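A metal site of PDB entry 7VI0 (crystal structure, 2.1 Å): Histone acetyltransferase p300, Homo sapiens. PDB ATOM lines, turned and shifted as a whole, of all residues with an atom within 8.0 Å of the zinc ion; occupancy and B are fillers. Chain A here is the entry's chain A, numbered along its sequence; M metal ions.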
ATOM      1  N   TYR A   6       4.210  27.686  -6.315  1.00  0.00           N
ATOM      2  CA  TYR A   6       3.344  27.304  -7.425  1.00  0.00           C
ATOM      3  C   TYR A   6       1.988  27.976  -7.294  1.00  0.00           C
ATOM      4  O   TYR A   6       1.452  28.088  -6.190  1.00  0.00           O
ATOM      5  CB  TYR A   6       3.198  25.789  -7.494  1.00  0.00           C
ATOM      6  N   CYS A   7       1.431  28.426  -8.424  1.00  0.00           N
ATOM      7  CA  CYS A   7       0.179  29.185  -8.426  1.00  0.00           C
ATOM      8  C   CYS A   7      -0.927  28.399  -7.743  1.00  0.00           C
ATOM      9  O   CYS A   7      -1.393  28.778  -6.666  1.00  0.00           O
ATOM     10  CB  CYS A   7      -0.216  29.526  -9.864  1.00  0.00           C
ATOM     11  SG  CYS A   7       0.048  28.148 -11.009  1.00  0.00           S
ATOM     12  N   CYS A   8      -1.331  27.294  -8.365  1.00  0.00           N
ATOM     13  CA  CYS A   8      -2.073  26.280  -7.628  1.00  0.00           C
ATOM     14  C   CYS A   8      -1.106  25.522  -6.716  1.00  0.00           C
ATOM     15  O   CYS A   8       0.117  25.583  -6.882  1.00  0.00           O
ATOM     16  CB  CYS A   8      -2.748  25.327  -8.606  1.00  0.00           C
ATOM     17  SG  CYS A   8      -1.621  24.740  -9.883  1.00  0.00           S
ATOM     18  N   GLY A   9      -1.663  24.765  -5.781  1.00  0.00           N
ATOM     19  CA  GLY A   9      -0.846  24.016  -4.854  1.00  0.00           C
ATOM     20  C   GLY A   9      -0.435  22.671  -5.423  1.00  0.00           C
ATOM     21  O   GLY A   9      -0.173  21.721  -4.669  1.00  0.00           O
ATOM     22  N   ARG A  10      -0.360  22.579  -6.743  1.00  0.00           N
ATOM     23  CA  ARG A  10      -0.344  21.302  -7.447  1.00  0.00           C
ATOM     24  C   ARG A  10       0.988  21.052  -8.124  1.00  0.00           C
ATOM     25  O   ARG A  10       1.543  21.941  -8.781  1.00  0.00           O
ATOM     26  CB  ARG A  10      -1.473  21.256  -8.486  1.00  0.00           C
ATOM     27  N   LYS A  11       1.493  19.827  -7.979  1.00  0.00           N
ATOM     28  CA  LYS A  11       2.669  19.359  -8.710  1.00  0.00           C
ATOM     29  C   LYS A  11       2.179  18.670  -9.985  1.00  0.00           C
ATOM     30  O   LYS A  11       1.551  17.611  -9.915  1.00  0.00           O
ATOM     31  CB  LYS A  11       3.509  18.418  -7.852  1.00  0.00           C
ATOM     32  CG  LYS A  11       4.941  18.229  -8.355  1.00  0.00           C
ATOM     33  CD  LYS A  11       5.388  16.772  -8.241  1.00  0.00           C
ATOM     34  CE  LYS A  11       6.842  16.610  -8.675  1.00  0.00           C
ATOM     35  NZ  LYS A  11       7.157  15.217  -9.106  1.00  0.00           N
ATOM     36  N   LEU A  12       2.481  19.260 -11.129  1.00  0.00           N
ATOM     37  CA  LEU A  12       1.890  18.860 -12.399  1.00  0.00           C
ATOM     38  C   LEU A  12       2.960  18.446 -13.390  1.00  0.00           C
ATOM     39  O   LEU A  12       4.010  19.080 -13.487  1.00  0.00           O
ATOM     40  CB  LEU A  12       1.044  19.995 -12.986  1.00  0.00           C
ATOM     41  CG  LEU A  12      -0.184  20.380 -12.160  1.00  0.00           C
ATOM     42  CD1 LEU A  12      -0.797  21.674 -12.678  1.00  0.00           C
ATOM     43  CD2 LEU A  12      -1.204  19.257 -12.151  1.00  0.00           C
ATOM     44  N   GLU A  86       5.595  20.270 -16.036  1.00  0.00           N
ATOM     45  CA  GLU A  86       5.024  21.437 -16.687  1.00  0.00           C
ATOM     46  C   GLU A  86       5.968  22.619 -16.535  1.00  0.00           C
ATOM     47  O   GLU A  86       6.762  22.708 -15.598  1.00  0.00           O
ATOM     48  CB  GLU A  86       3.656  21.766 -16.086  1.00  0.00           C
ATOM     49  CG  GLU A  86       2.514  20.911 -16.636  1.00  0.00           C
ATOM     50  CD  GLU A  86       1.154  21.530 -16.406  1.00  0.00           C
ATOM     51  OE1 GLU A  86       1.074  22.772 -16.237  1.00  0.00           O
ATOM     52  OE2 GLU A  86       0.160  20.782 -16.395  1.00  0.00           O
ATOM     53  N   LEU A  87       5.874  23.547 -17.486  1.00  0.00           N
ATOM     54  CA  LEU A  87       6.753  24.710 -17.486  1.00  0.00           C
ATOM     55  C   LEU A  87       6.160  25.824 -16.648  1.00  0.00           C
ATOM     56  O   LEU A  87       4.936  25.953 -16.511  1.00  0.00           O
ATOM     57  CB  LEU A  87       6.992  25.194 -18.922  1.00  0.00           C
ATOM     58  CG  LEU A  87       7.583  24.191 -19.908  1.00  0.00           C
ATOM     59  CD1 LEU A  87       8.170  24.894 -21.118  1.00  0.00           C
ATOM     60  CD2 LEU A  87       8.628  23.312 -19.233  1.00  0.00           C
ATOM     61  N   PHE A  88       7.034  26.641 -16.075  1.00  0.00           N
ATOM     62  CA  PHE A  88       6.657  27.823 -15.323  1.00  0.00           C
ATOM     63  C   PHE A  88       7.030  29.073 -16.094  1.00  0.00           C
ATOM     64  O   PHE A  88       7.958  29.078 -16.905  1.00  0.00           O
ATOM     65  CB  PHE A  88       7.336  27.852 -13.953  1.00  0.00           C
ATOM     66  CG  PHE A  88       6.879  26.765 -13.016  1.00  0.00           C
ATOM     67  CD1 PHE A  88       7.314  25.459 -13.194  1.00  0.00           C
ATOM     68  CD2 PHE A  88       6.017  27.046 -11.972  1.00  0.00           C
ATOM     69  CE1 PHE A  88       6.895  24.455 -12.335  1.00  0.00           C
ATOM     70  CE2 PHE A  88       5.598  26.042 -11.113  1.00  0.00           C
ATOM     71  CZ  PHE A  88       6.047  24.744 -11.297  1.00  0.00           C
ATOM     72  N   LYS A  97       6.284  32.782  -9.754  1.00  0.00           N
ATOM     73  CA  LYS A  97       6.360  31.688 -10.709  1.00  0.00           C
ATOM     74  C   LYS A  97       5.012  31.004 -10.783  1.00  0.00           C
ATOM     75  O   LYS A  97       4.457  30.615  -9.750  1.00  0.00           O
ATOM     76  CB  LYS A  97       7.454  30.689 -10.319  1.00  0.00           C
ATOM     77  CG  LYS A  97       8.811  30.975 -10.963  1.00  0.00           C
ATOM     78  CD  LYS A  97       9.836  29.909 -10.575  1.00  0.00           C
ATOM     79  CE  LYS A  97      11.219  30.509 -10.374  1.00  0.00           C
ATOM     80  NZ  LYS A  97      11.954  29.867  -9.254  1.00  0.00           N
ATOM     81  N   MET A  98       4.471  30.874 -11.990  1.00  0.00           N
ATOM     82  CA  MET A  98       3.206  30.211 -12.217  1.00  0.00           C
ATOM     83  C   MET A  98       3.337  29.211 -13.359  1.00  0.00           C
ATOM     84  O   MET A  98       4.145  29.408 -14.270  1.00  0.00           O
ATOM     85  CB  MET A  98       2.084  31.212 -12.573  1.00  0.00           C
ATOM     86  CG  MET A  98       2.298  32.616 -12.050  1.00  0.00           C
ATOM     87  SD  MET A  98       1.459  32.881 -10.485  1.00  0.00           S
ATOM     88  CE  MET A  98      -0.141  33.451 -11.041  1.00  0.00           C
ATOM     89  N   HIS A  99       2.551  28.145 -13.298  1.00  0.00           N
ATOM     90  CA  HIS A  99       2.418  27.262 -14.446  1.00  0.00           C
ATOM     91  C   HIS A  99       2.011  28.083 -15.658  1.00  0.00           C
ATOM     92  O   HIS A  99       1.089  28.886 -15.584  1.00  0.00           O
ATOM     93  CB  HIS A  99       1.378  26.182 -14.170  1.00  0.00           C
ATOM     94  CG  HIS A  99       1.770  25.189 -13.118  1.00  0.00           C
ATOM     95  ND1 HIS A  99       1.034  24.998 -11.962  1.00  0.00           N
ATOM     96  CD2 HIS A  99       2.803  24.326 -13.054  1.00  0.00           C
ATOM     97  CE1 HIS A  99       1.609  24.058 -11.232  1.00  0.00           C
ATOM     98  NE2 HIS A  99       2.688  23.630 -11.871  1.00  0.00           N
ATOM     99  N   GLN A 100       2.726  27.881 -16.764  1.00  0.00           N
ATOM    100  CA  GLN A 100       2.383  28.606 -17.987  1.00  0.00           C
ATOM    101  C   GLN A 100       0.957  28.302 -18.425  1.00  0.00           C
ATOM    102  O   GLN A 100       0.233  29.190 -18.886  1.00  0.00           O
ATOM    103  CB  GLN A 100       3.372  28.256 -19.107  1.00  0.00           C
ATOM    104  CG  GLN A 100       3.237  29.134 -20.341  1.00  0.00           C
ATOM    105  CD  GLN A 100       4.317  28.857 -21.371  1.00  0.00           C
ATOM    106  OE1 GLN A 100       4.980  27.828 -21.339  1.00  0.00           O
ATOM    107  NE2 GLN A 100       4.484  29.790 -22.308  1.00  0.00           N
ATOM    108  N   ILE A 101       0.523  27.046 -18.259  1.00  0.00           N
ATOM    109  CA  ILE A 101      -0.816  26.656 -18.661  1.00  0.00           C
ATOM    110  C   ILE A 101      -1.868  27.306 -17.773  1.00  0.00           C
ATOM    111  O   ILE A 101      -2.947  27.682 -18.233  1.00  0.00           O
ATOM    112  CB  ILE A 101      -0.926  25.113 -18.640  1.00  0.00           C
ATOM    113  CG1 ILE A 101      -0.008  24.514 -19.713  1.00  0.00           C
ATOM    114  CG2 ILE A 101      -2.364  24.670 -18.853  1.00  0.00           C
ATOM    115  CD1 ILE A 101       0.029  22.994 -19.715  1.00  0.00           C
ATOM    116  N   CYS A 102      -1.561  27.474 -16.476  1.00  0.00           N
ATOM    117  CA  CYS A 102      -2.540  28.031 -15.546  1.00  0.00           C
ATOM    118  C   CYS A 102      -2.884  29.483 -15.883  1.00  0.00           C
ATOM    119  O   CYS A 102      -4.040  29.882 -15.803  1.00  0.00           O
ATOM    120  CB  CYS A 102      -2.025  27.923 -14.113  1.00  0.00           C
ATOM    121  SG  CYS A 102      -2.293  26.321 -13.340  1.00  0.00           S
ATOM    122  N   VAL A 103      -1.879  30.274 -16.260  1.00  0.00           N
ATOM    123  CA  VAL A 103      -2.095  31.683 -16.557  1.00  0.00           C
ATOM    124  C   VAL A 103      -2.230  31.955 -18.049  1.00  0.00           C
ATOM    125  O   VAL A 103      -2.489  33.096 -18.438  1.00  0.00           O
ATOM    126  CB  VAL A 103      -0.971  32.557 -15.958  1.00  0.00           C
ATOM    127  CG1 VAL A 103      -1.019  32.506 -14.445  1.00  0.00           C
ATOM    128  CG2 VAL A 103       0.389  32.105 -16.466  1.00  0.00           C
ATOM    129  N   ARG A 433      -7.986  22.867 -18.386  1.00  0.00           N
ATOM    130  CA  ARG A 433      -6.902  23.836 -18.421  1.00  0.00           C
ATOM    131  C   ARG A 433      -5.903  23.535 -19.536  1.00  0.00           C
ATOM    132  O   ARG A 433      -5.459  24.451 -20.229  1.00  0.00           O
ATOM    133  CB  ARG A 433      -6.201  23.904 -17.064  1.00  0.00           C
ATOM    134  CG  ARG A 433      -5.700  22.577 -16.504  1.00  0.00           C
ATOM    135  CD  ARG A 433      -5.070  22.752 -15.136  1.00  0.00           C
ATOM    136  NE  ARG A 433      -3.913  23.642 -15.158  1.00  0.00           N
ATOM    137  CZ  ARG A 433      -2.687  23.272 -15.508  1.00  0.00           C
ATOM    138  NH1 ARG A 433      -2.422  22.027 -15.889  1.00  0.00           N
ATOM    139  NH2 ARG A 433      -1.710  24.163 -15.482  1.00  0.00           N
HETATM  140 ZN    ZN M   1      -0.770  26.055 -11.595  1.00  0.00          ZN
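NH2 of Arg 433 lies close to SG of Cys 102, at 3.1 Å.
Four residues have an atom within 4 Å of the zinc ion: Cys 7, Cys 8, His 99 and Cys 102.
ND1 of His 99 binds the zinc ion (2.1 Å). SG of Cys 8 is bound to the zinc ion, at 2.3 Å. SG of Cys 7 binds the zinc ion (2.3 Å). SG of Cys 102 is bound to the zinc ion, 2.3 Å away.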
